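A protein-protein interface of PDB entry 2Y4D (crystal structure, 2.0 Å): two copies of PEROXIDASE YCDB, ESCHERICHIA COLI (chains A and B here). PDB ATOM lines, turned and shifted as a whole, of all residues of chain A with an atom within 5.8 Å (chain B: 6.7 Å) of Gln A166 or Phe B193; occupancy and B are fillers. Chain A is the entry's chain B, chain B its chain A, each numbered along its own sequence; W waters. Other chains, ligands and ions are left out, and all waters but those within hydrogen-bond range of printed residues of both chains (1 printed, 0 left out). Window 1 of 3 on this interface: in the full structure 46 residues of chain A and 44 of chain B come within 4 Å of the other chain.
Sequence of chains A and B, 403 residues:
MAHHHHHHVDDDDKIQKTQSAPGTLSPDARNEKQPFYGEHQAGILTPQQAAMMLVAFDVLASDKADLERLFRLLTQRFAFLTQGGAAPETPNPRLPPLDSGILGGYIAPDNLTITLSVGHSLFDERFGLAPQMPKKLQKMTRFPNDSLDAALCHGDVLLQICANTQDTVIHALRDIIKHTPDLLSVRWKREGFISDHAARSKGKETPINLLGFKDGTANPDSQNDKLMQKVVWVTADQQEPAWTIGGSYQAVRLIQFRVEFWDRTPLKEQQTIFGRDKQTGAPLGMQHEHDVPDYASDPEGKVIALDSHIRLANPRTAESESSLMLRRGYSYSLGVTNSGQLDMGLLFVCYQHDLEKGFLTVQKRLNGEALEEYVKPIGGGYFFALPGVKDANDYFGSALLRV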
ATOM      1  N   ALA A  51      21.106  -5.781 -21.852  1.00  0.00           N
ATOM      2  CA  ALA A  51      20.444  -5.616 -20.559  1.00  0.00           C
ATOM      3  C   ALA A  51      19.900  -6.947 -20.059  1.00  0.00           C
ATOM      4  O   ALA A  51      19.500  -7.839 -20.842  1.00  0.00           O
ATOM      5  CB  ALA A  51      19.336  -4.559 -20.638  1.00  0.00           C
ATOM      6  N   ASP A 110      12.612  -6.359 -29.238  1.00  0.00           N
ATOM      7  CA  ASP A 110      13.881  -5.861 -28.705  1.00  0.00           C
ATOM      8  C   ASP A 110      14.817  -7.008 -28.252  1.00  0.00           C
ATOM      9  O   ASP A 110      15.416  -6.948 -27.168  1.00  0.00           O
ATOM     10  CB  ASP A 110      13.562  -4.917 -27.537  1.00  0.00           C
ATOM     11  CG  ASP A 110      14.657  -3.900 -27.267  1.00  0.00           C
ATOM     12  OD1 ASP A 110      15.303  -3.414 -28.225  1.00  0.00           O
ATOM     13  OD2 ASP A 110      14.832  -3.561 -26.075  1.00  0.00           O
ATOM     14  N   ALA A 163      17.248  -8.497 -22.763  1.00  0.00           N
ATOM     15  CA  ALA A 163      16.812  -7.733 -23.957  1.00  0.00           C
ATOM     16  C   ALA A 163      17.868  -6.701 -24.290  1.00  0.00           C
ATOM     17  O   ALA A 163      18.823  -6.520 -23.502  1.00  0.00           O
ATOM     18  CB  ALA A 163      15.459  -7.070 -23.748  1.00  0.00           C
ATOM     19  N   ASN A 164      17.752  -6.076 -25.465  1.00  0.00           N
ATOM     20  CA  ASN A 164      18.594  -4.915 -25.803  1.00  0.00           C
ATOM     21  C   ASN A 164      18.539  -3.802 -24.768  1.00  0.00           C
ATOM     22  O   ASN A 164      19.524  -3.108 -24.538  1.00  0.00           O
ATOM     23  CB  ASN A 164      18.255  -4.300 -27.186  1.00  0.00           C
ATOM     24  CG  ASN A 164      18.301  -5.293 -28.305  1.00  0.00           C
ATOM     25  OD1 ASN A 164      19.120  -6.200 -28.310  1.00  0.00           O
ATOM     26  ND2 ASN A 164      17.390  -5.138 -29.282  1.00  0.00           N
ATOM     27  N   THR A 165      17.379  -3.579 -24.171  1.00  0.00           N
ATOM     28  CA  THR A 165      17.268  -2.438 -23.278  1.00  0.00           C
ATOM     29  C   THR A 165      16.671  -2.860 -21.946  1.00  0.00           C
ATOM     30  O   THR A 165      15.959  -3.864 -21.856  1.00  0.00           O
ATOM     31  CB  THR A 165      16.383  -1.330 -23.860  1.00  0.00           C
ATOM     32  OG1 THR A 165      15.104  -1.886 -24.175  1.00  0.00           O
ATOM     33  CG2 THR A 165      16.981  -0.690 -25.131  1.00  0.00           C
ATOM     34  N   GLN A 166      16.954  -2.059 -20.924  1.00  0.00           N
ATOM     35  CA  GLN A 166      16.419  -2.264 -19.587  1.00  0.00           C
ATOM     36  C   GLN A 166      14.866  -2.097 -19.512  1.00  0.00           C
ATOM     37  O   GLN A 166      14.215  -2.763 -18.735  1.00  0.00           O
ATOM     38  CB  GLN A 166      17.111  -1.269 -18.658  1.00  0.00           C
ATOM     39  CG  GLN A 166      16.668  -1.247 -17.220  1.00  0.00           C
ATOM     40  CD  GLN A 166      17.630  -0.417 -16.345  1.00  0.00           C
ATOM     41  OE1 GLN A 166      18.350   0.434 -16.852  1.00  0.00           O
ATOM     42  NE2 GLN A 166      17.610  -0.653 -15.039  1.00  0.00           N
ATOM     43  N   ASP A 167      14.330  -1.159 -20.293  1.00  0.00           N
ATOM     44  CA  ASP A 167      12.893  -0.863 -20.400  1.00  0.00           C
ATOM     45  C   ASP A 167      12.107  -2.149 -20.694  1.00  0.00           C
ATOM     46  O   ASP A 167      11.116  -2.450 -20.031  1.00  0.00           O
ATOM     47  CB  ASP A 167      12.670   0.039 -21.630  1.00  0.00           C
ATOM     48  CG  ASP A 167      12.688   1.508 -21.322  1.00  0.00           C
ATOM     49  OD1 ASP A 167      13.777   2.085 -21.053  1.00  0.00           O
ATOM     50  OD2 ASP A 167      11.605   2.118 -21.412  1.00  0.00           O
ATOM     51  N   THR A 168      12.547  -2.871 -21.727  1.00  0.00           N
ATOM     52  CA  THR A 168      11.880  -4.067 -22.200  1.00  0.00           C
ATOM     53  C   THR A 168      11.848  -5.138 -21.116  1.00  0.00           C
ATOM     54  O   THR A 168      10.832  -5.811 -20.906  1.00  0.00           O
ATOM     55  CB  THR A 168      12.653  -4.638 -23.448  1.00  0.00           C
ATOM     56  OG1 THR A 168      12.661  -3.658 -24.480  1.00  0.00           O
ATOM     57  CG2 THR A 168      12.052  -5.925 -23.965  1.00  0.00           C
ATOM     58  N   VAL A 169      12.990  -5.301 -20.436  1.00  0.00           N
ATOM     59  CA  VAL A 169      13.143  -6.291 -19.376  1.00  0.00           C
ATOM     60  C   VAL A 169      12.193  -5.977 -18.195  1.00  0.00           C
ATOM     61  O   VAL A 169      11.562  -6.859 -17.630  1.00  0.00           O
ATOM     62  CB  VAL A 169      14.657  -6.288 -18.926  1.00  0.00           C
ATOM     63  CG1 VAL A 169      14.854  -7.060 -17.681  1.00  0.00           C
ATOM     64  CG2 VAL A 169      15.538  -6.868 -20.073  1.00  0.00           C
ATOM     65  N   ILE A 170      12.109  -4.715 -17.812  1.00  0.00           N
ATOM     66  CA  ILE A 170      11.266  -4.325 -16.688  1.00  0.00           C
ATOM     67  C   ILE A 170       9.793  -4.441 -17.102  1.00  0.00           C
ATOM     68  O   ILE A 170       8.948  -4.858 -16.314  1.00  0.00           O
ATOM     69  CB  ILE A 170      11.540  -2.876 -16.224  1.00  0.00           C
ATOM     70  CG1 ILE A 170      12.900  -2.792 -15.497  1.00  0.00           C
ATOM     71  CG2 ILE A 170      10.390  -2.395 -15.329  1.00  0.00           C
ATOM     72  CD1 ILE A 170      13.453  -1.317 -15.387  1.00  0.00           C
ATOM     73  N   HIS A 171       9.498  -4.061 -18.334  1.00  0.00           N
ATOM     74  CA  HIS A 171       8.136  -4.274 -18.881  1.00  0.00           C
ATOM     75  C   HIS A 171       7.736  -5.762 -18.823  1.00  0.00           C
ATOM     76  O   HIS A 171       6.625  -6.087 -18.361  1.00  0.00           O
ATOM     77  CB  HIS A 171       8.026  -3.753 -20.321  1.00  0.00           C
ATOM     78  CG  HIS A 171       6.691  -4.042 -20.920  1.00  0.00           C
ATOM     79  ND1 HIS A 171       6.442  -5.187 -21.638  1.00  0.00           N
ATOM     80  CD2 HIS A 171       5.507  -3.403 -20.798  1.00  0.00           C
ATOM     81  CE1 HIS A 171       5.156  -5.227 -21.956  1.00  0.00           C
ATOM     82  NE2 HIS A 171       4.569  -4.159 -21.454  1.00  0.00           N
ATOM     83  N   GLU A 191      19.550  -6.614 -11.479  1.00  0.00           N
ATOM     84  CA  GLU A 191      19.646  -6.207 -12.873  1.00  0.00           C
ATOM     85  C   GLU A 191      21.116  -5.986 -13.241  1.00  0.00           C
ATOM     86  O   GLU A 191      21.893  -5.519 -12.409  1.00  0.00           O
ATOM     87  CB  GLU A 191      18.821  -4.928 -13.112  1.00  0.00           C
ATOM     88  CG  GLU A 191      17.301  -5.228 -12.988  1.00  0.00           C
ATOM     89  CD  GLU A 191      16.388  -4.096 -13.471  1.00  0.00           C
ATOM     90  OE1 GLU A 191      16.616  -3.517 -14.549  1.00  0.00           O
ATOM     91  OE2 GLU A 191      15.417  -3.807 -12.784  1.00  0.00           O
ATOM     92  N   GLN B  49      20.444  12.496 -21.298  1.00  0.00           N
ATOM     93  CA  GLN B  49      21.120  11.331 -21.830  1.00  0.00           C
ATOM     94  C   GLN B  49      20.446  10.132 -21.186  1.00  0.00           C
ATOM     95  O   GLN B  49      19.787  10.305 -20.150  1.00  0.00           O
ATOM     96  CB  GLN B  49      22.592  11.324 -21.422  1.00  0.00           C
ATOM     97  CG  GLN B  49      23.361  12.626 -21.791  1.00  0.00           C
ATOM     98  CD  GLN B  49      23.459  13.599 -20.635  1.00  0.00           C
ATOM     99  OE1 GLN B  49      22.480  13.846 -19.909  1.00  0.00           O
ATOM    100  NE2 GLN B  49      24.639  14.190 -20.456  1.00  0.00           N
ATOM    101  N   ALA B  50      20.661   8.946 -21.754  1.00  0.00           N
ATOM    102  CA  ALA B  50      19.964   7.734 -21.310  1.00  0.00           C
ATOM    103  C   ALA B  50      20.428   7.198 -19.943  1.00  0.00           C
ATOM    104  O   ALA B  50      19.680   6.517 -19.281  1.00  0.00           O
ATOM    105  CB  ALA B  50      20.073   6.619 -22.367  1.00  0.00           C
ATOM    106  N   ALA B  51      21.654   7.481 -19.533  1.00  0.00           N
ATOM    107  CA  ALA B  51      22.122   6.891 -18.253  1.00  0.00           C
ATOM    108  C   ALA B  51      22.513   7.962 -17.272  1.00  0.00           C
ATOM    109  O   ALA B  51      23.052   9.018 -17.645  1.00  0.00           O
ATOM    110  CB  ALA B  51      23.262   5.898 -18.475  1.00  0.00           C
ATOM    111  N   MET B  52      22.287   7.688 -15.987  1.00  0.00           N
ATOM    112  CA  MET B  52      22.577   8.688 -14.983  1.00  0.00           C
ATOM    113  C   MET B  52      22.970   8.024 -13.656  1.00  0.00           C
ATOM    114  O   MET B  52      22.582   6.887 -13.391  1.00  0.00           O
ATOM    115  CB  MET B  52      21.354   9.606 -14.761  1.00  0.00           C
ATOM    116  CG  MET B  52      21.723  10.913 -14.070  1.00  0.00           C
ATOM    117  SD  MET B  52      21.199  11.124 -12.373  1.00  0.00           S
ATOM    118  CE  MET B  52      20.065  12.475 -12.576  1.00  0.00           C
ATOM    119  N   GLN B 166      25.719   3.427 -19.284  1.00  0.00           N
ATOM    120  CA  GLN B 166      26.062   3.237 -17.892  1.00  0.00           C
ATOM    121  C   GLN B 166      27.586   3.011 -17.750  1.00  0.00           C
ATOM    122  O   GLN B 166      28.179   3.402 -16.754  1.00  0.00           O
ATOM    123  CB  GLN B 166      25.295   2.010 -17.432  1.00  0.00           C
ATOM    124  CG  GLN B 166      25.635   1.397 -16.125  1.00  0.00           C
ATOM    125  CD  GLN B 166      24.452   0.512 -15.627  1.00  0.00           C
ATOM    126  OE1 GLN B 166      23.783  -0.142 -16.437  1.00  0.00           O
ATOM    127  NE2 GLN B 166      24.186   0.534 -14.300  1.00  0.00           N
ATOM    128  N   GLU B 191      21.711   4.852  -9.370  1.00  0.00           N
ATOM    129  CA  GLU B 191      21.812   4.937 -10.806  1.00  0.00           C
ATOM    130  C   GLU B 191      20.414   4.924 -11.421  1.00  0.00           C
ATOM    131  O   GLU B 191      19.504   4.215 -10.921  1.00  0.00           O
ATOM    132  CB  GLU B 191      22.636   3.774 -11.337  1.00  0.00           C
ATOM    133  CG  GLU B 191      24.131   3.914 -10.902  1.00  0.00           C
ATOM    134  CD  GLU B 191      25.098   2.992 -11.662  1.00  0.00           C
ATOM    135  OE1 GLU B 191      24.925   2.740 -12.872  1.00  0.00           O
ATOM    136  OE2 GLU B 191      26.086   2.570 -11.049  1.00  0.00           O
ATOM    137  N   GLY B 192      20.247   5.680 -12.511  1.00  0.00           N
ATOM    138  CA  GLY B 192      18.958   5.755 -13.161  1.00  0.00           C
ATOM    139  C   GLY B 192      19.050   5.822 -14.675  1.00  0.00           C
ATOM    140  O   GLY B 192      20.138   5.846 -15.224  1.00  0.00           O
ATOM    141  N   PHE B 193      17.885   5.862 -15.323  1.00  0.00           N
ATOM    142  CA  PHE B 193      17.796   5.811 -16.779  1.00  0.00           C
ATOM    143  C   PHE B 193      16.528   6.498 -17.285  1.00  0.00           C
ATOM    144  O   PHE B 193      15.587   6.720 -16.524  1.00  0.00           O
ATOM    145  CB  PHE B 193      17.801   4.360 -17.253  1.00  0.00           C
ATOM    146  CG  PHE B 193      16.587   3.568 -16.808  1.00  0.00           C
ATOM    147  CD1 PHE B 193      16.537   2.999 -15.529  1.00  0.00           C
ATOM    148  CD2 PHE B 193      15.497   3.398 -17.666  1.00  0.00           C
ATOM    149  CE1 PHE B 193      15.405   2.258 -15.106  1.00  0.00           C
ATOM    150  CE2 PHE B 193      14.355   2.675 -17.257  1.00  0.00           C
ATOM    151  CZ  PHE B 193      14.316   2.108 -15.973  1.00  0.00           C
ATOM    152  N   ILE B 194      16.546   6.877 -18.551  1.00  0.00           N
ATOM    153  CA  ILE B 194      15.277   7.130 -19.292  1.00  0.00           C
ATOM    154  C   ILE B 194      15.278   6.224 -20.527  1.00  0.00           C
ATOM    155  O   ILE B 194      16.295   5.607 -20.840  1.00  0.00           O
ATOM    156  CB  ILE B 194      15.158   8.609 -19.690  1.00  0.00           C
ATOM    157  CG1 ILE B 194      16.352   9.050 -20.566  1.00  0.00           C
ATOM    158  CG2 ILE B 194      15.015   9.480 -18.454  1.00  0.00           C
ATOM    159  CD1 ILE B 194      16.058  10.370 -21.424  1.00  0.00           C
ATOM    160  N   SER B 195      14.187   6.124 -21.272  1.00  0.00           N
ATOM    161  CA  SER B 195      14.290   5.314 -22.516  1.00  0.00           C
ATOM    162  C   SER B 195      15.259   5.882 -23.567  1.00  0.00           C
ATOM    163  O   SER B 195      15.476   7.094 -23.677  1.00  0.00           O
ATOM    164  CB  SER B 195      12.944   5.095 -23.161  1.00  0.00           C
ATOM    165  OG  SER B 195      12.468   6.337 -23.666  1.00  0.00           O
ATOM    166  N   ASP B 196      15.842   4.988 -24.350  1.00  0.00           N
ATOM    167  CA  ASP B 196      16.719   5.415 -25.443  1.00  0.00           C
ATOM    168  C   ASP B 196      15.957   6.214 -26.510  1.00  0.00           C
ATOM    169  O   ASP B 196      16.490   7.208 -27.051  1.00  0.00           O
ATOM    170  CB  ASP B 196      17.455   4.203 -26.033  1.00  0.00           C
ATOM    171  CG  ASP B 196      18.685   3.807 -25.205  1.00  0.00           C
ATOM    172  OD1 ASP B 196      19.685   4.577 -25.201  1.00  0.00           O
ATOM    173  OD2 ASP B 196      18.663   2.727 -24.571  1.00  0.00           O
ATOM    174  N   PRO B 207      10.073  11.584 -21.639  1.00  0.00           N
ATOM    175  CA  PRO B 207      10.309  10.268 -21.040  1.00  0.00           C
ATOM    176  C   PRO B 207       9.074   9.773 -20.308  1.00  0.00           C
ATOM    177  O   PRO B 207       8.360  10.566 -19.731  1.00  0.00           O
ATOM    178  CB  PRO B 207      11.420  10.547 -20.016  1.00  0.00           C
ATOM    179  CG  PRO B 207      12.100  11.763 -20.507  1.00  0.00           C
ATOM    180  CD  PRO B 207      10.995  12.601 -21.102  1.00  0.00           C
ATOM    181  N   ILE B 208       8.818   8.471 -20.345  1.00  0.00           N
ATOM    182  CA  ILE B 208       7.708   7.884 -19.582  1.00  0.00           C
ATOM    183  C   ILE B 208       8.302   7.330 -18.297  1.00  0.00           C
ATOM    184  O   ILE B 208       9.323   6.632 -18.319  1.00  0.00           O
ATOM    185  CB  ILE B 208       7.002   6.776 -20.361  1.00  0.00           C
ATOM    186  CG1 ILE B 208       6.389   7.327 -21.676  1.00  0.00           C
ATOM    187  CG2 ILE B 208       5.913   6.100 -19.509  1.00  0.00           C
ATOM    188  CD1 ILE B 208       6.105   6.236 -22.681  1.00  0.00           C
ATOM    189  N   LEU B 210       8.035   5.134 -14.469  1.00  0.00           N
ATOM    190  CA  LEU B 210       7.697   3.731 -14.185  1.00  0.00           C
ATOM    191  C   LEU B 210       6.219   3.495 -13.795  1.00  0.00           C
ATOM    192  O   LEU B 210       5.809   2.357 -13.598  1.00  0.00           O
ATOM    193  CB  LEU B 210       8.689   3.055 -13.210  1.00  0.00           C
ATOM    194  CG  LEU B 210      10.031   2.725 -13.900  1.00  0.00           C
ATOM    195  CD1 LEU B 210      11.190   2.446 -12.866  1.00  0.00           C
ATOM    196  CD2 LEU B 210       9.973   1.588 -14.960  1.00  0.00           C
ATOM    197  N   GLY B 329      14.307  14.510 -14.184  1.00  0.00           N
ATOM    198  CA  GLY B 329      14.262  13.243 -13.421  1.00  0.00           C
ATOM    199  C   GLY B 329      14.523  11.977 -14.226  1.00  0.00           C
ATOM    200  O   GLY B 329      14.345  11.966 -15.465  1.00  0.00           O
ATOM    201  N   TYR B 330      14.963  10.906 -13.535  1.00  0.00           N
ATOM    202  CA  TYR B 330      15.273   9.628 -14.181  1.00  0.00           C
ATOM    203  C   TYR B 330      14.558   8.503 -13.443  1.00  0.00           C
ATOM    204  O   TYR B 330      14.382   8.587 -12.215  1.00  0.00           O
ATOM    205  CB  TYR B 330      16.793   9.358 -14.131  1.00  0.00           C
ATOM    206  CG  TYR B 330      17.599  10.132 -15.173  1.00  0.00           C
ATOM    207  CD1 TYR B 330      17.901  11.501 -15.000  1.00  0.00           C
ATOM    208  CD2 TYR B 330      18.097   9.477 -16.293  1.00  0.00           C
ATOM    209  CE1 TYR B 330      18.678  12.199 -15.977  1.00  0.00           C
ATOM    210  CE2 TYR B 330      18.852  10.144 -17.266  1.00  0.00           C
ATOM    211  CZ  TYR B 330      19.129  11.504 -17.102  1.00  0.00           C
ATOM    212  OH  TYR B 330      19.879  12.145 -18.069  1.00  0.00           O
ATOM    213  N   SER B 331      14.213   7.443 -14.156  1.00  0.00           N
ATOM    214  CA  SER B 331      13.663   6.245 -13.507  1.00  0.00           C
ATOM    215  C   SER B 331      14.767   5.450 -12.810  1.00  0.00           C
ATOM    216  O   SER B 331      15.944   5.576 -13.168  1.00  0.00           O
ATOM    217  CB  SER B 331      13.003   5.372 -14.556  1.00  0.00           C
ATOM    218  OG  SER B 331      11.871   6.056 -15.075  1.00  0.00           O
ATOM    219  N   TYR B 332      14.403   4.624 -11.816  1.00  0.00           N
ATOM    220  CA  TYR B 332      15.410   3.721 -11.255  1.00  0.00           C
ATOM    221  C   TYR B 332      14.768   2.385 -10.961  1.00  0.00           C
ATOM    222  O   TYR B 332      13.569   2.323 -10.681  1.00  0.00           O
ATOM    223  CB  TYR B 332      16.095   4.317  -9.984  1.00  0.00           C
ATOM    224  CG  TYR B 332      15.333   4.208  -8.693  1.00  0.00           C
ATOM    225  CD1 TYR B 332      15.307   3.006  -7.942  1.00  0.00           C
ATOM    226  CD2 TYR B 332      14.630   5.303  -8.195  1.00  0.00           C
ATOM    227  CE1 TYR B 332      14.559   2.919  -6.751  1.00  0.00           C
ATOM    228  CE2 TYR B 332      13.939   5.218  -6.963  1.00  0.00           C
ATOM    229  CZ  TYR B 332      13.915   4.021  -6.279  1.00  0.00           C
ATOM    230  OH  TYR B 332      13.231   3.992  -5.092  1.00  0.00           O
ATOM    231  N   SER B 333      15.568   1.326 -11.007  1.00  0.00           N
ATOM    232  CA  SER B 333      15.058   0.012 -10.707  1.00  0.00           C
ATOM    233  C   SER B 333      16.155  -0.770 -10.080  1.00  0.00           C
ATOM    234  O   SER B 333      17.194  -1.002 -10.708  1.00  0.00           O
ATOM    235  CB  SER B 333      14.588  -0.716 -11.968  1.00  0.00           C
ATOM    236  OG  SER B 333      13.997  -1.969 -11.637  1.00  0.00           O
ATOM    237  N   LEU B 334      15.912  -1.242  -8.857  1.00  0.00           N
ATOM    238  CA  LEU B 334      16.986  -1.877  -8.088  1.00  0.00           C
ATOM    239  C   LEU B 334      16.701  -3.343  -7.809  1.00  0.00           C
ATOM    240  O   LEU B 334      16.652  -4.156  -8.736  1.00  0.00           O
ATOM    241  CB  LEU B 334      17.266  -1.084  -6.808  1.00  0.00           C
ATOM    242  CG  LEU B 334      17.515   0.424  -6.905  1.00  0.00           C
ATOM    243  CD1 LEU B 334      17.992   0.950  -5.561  1.00  0.00           C
ATOM    244  CD2 LEU B 334      18.568   0.745  -8.000  1.00  0.00           C
ATOM    245  N   GLY B 345      11.467   3.384  -8.823  1.00  0.00           N
ATOM    246  CA  GLY B 345      10.812   4.668  -8.698  1.00  0.00           C
ATOM    247  C   GLY B 345      11.441   5.765  -9.528  1.00  0.00           C
ATOM    248  O   GLY B 345      11.737   5.576 -10.705  1.00  0.00           O
ATOM    249  N   LEU B 347      14.276   9.112  -9.565  1.00  0.00           N
ATOM    250  CA  LEU B 347      15.320  10.008  -9.057  1.00  0.00           C
ATOM    251  C   LEU B 347      14.932  11.370  -9.541  1.00  0.00           C
ATOM    252  O   LEU B 347      15.262  11.726 -10.675  1.00  0.00           O
ATOM    253  CB  LEU B 347      16.712   9.627  -9.591  1.00  0.00           C
ATOM    254  CG  LEU B 347      17.032   8.162  -9.358  1.00  0.00           C
ATOM    255  CD1 LEU B 347      18.374   7.775 -10.028  1.00  0.00           C
ATOM    256  CD2 LEU B 347      17.018   7.759  -7.790  1.00  0.00           C
HETATM  257  O   HOH W   1      19.371  -4.567  -9.403  1.00  0.00           O
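The side-chain hydroxyl of Ser B333 sits at hydrogen-bond distance from the side-chain carboxylate of Glu A191.
The backbone carbonyl oxygen of Phe B193 is in hydrogen-bond range of the backbone NH of Ser B331, at 2.8 Å. OG1 of Thr A165 lies within hydrogen-bond range of OD2 of Asp A110 (2.5 Å). The side-chain hydroxyl of Thr A165 sits at hydrogen-bond distance from the side-chain hydroxyl of Thr A168, at 3.0 Å. The side-chain amide nitrogen of Gln A166 is in hydrogen-bond range of the side-chain carboxylate of Glu A191, at 3.1 Å.
Among the printed residues, merely in contact across the chains: Gln A166 with Phe B193, Ile A170 with Phe B193, Asp A167 with Ser B195, Ile A170 with Ser B333, Thr A165 with Asp B196 and Asp A167 with Phe B193.
Gln A166 touches just one residue of chain B: Phe B193. Phe B193 touches three residues of chain A. Of the printed residues of chain A, Asp B196 touches Thr A165. Of the printed residues of chain B, Glu A191 touches Ser B333. Printed residues of chain B within 4 Å of Thr A165: Asp B196 (3.8 Å). Printed residues of chain A within 4 Å of Ser B333: Ile A170 (3.7 Å) and Glu A191 (2.6 Å). Ile B194 touches none of the printed residues of chain A. Tyr B332 touches none of the printed residues of chain A. The nearest residue of chain B that does not touch Gln A166 is Ser B333 (4.3 Å).
Of the 22 printed residues of chain B, 4 touch a printed residue of chain A. Of the 12 printed residues of chain A, 5 touch a printed residue of chain B. Hydrophobic or aromatic side chains of chain A within 4 Å of the printed part of chain B: Ile A170. Along chain A the printed residues that touch a printed residue of chain B span positions 165 to 191. Among the printed residues, no Asp or Glu carboxylate lies within 4 Å of a Lys or Arg side-chain nitrogen of the other chain.
Positions printed for both chains: 51, 166 and 191. Of the 7 pairs that touch across the chains among the printed residues, none has its exchanged pair printed and touching as well.
Water W1 lies within hydrogen-bond range of the backbone carbonyl oxygen of Leu B334 (2.8 Å) and the backbone NH of Glu A191 (2.9 Å).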
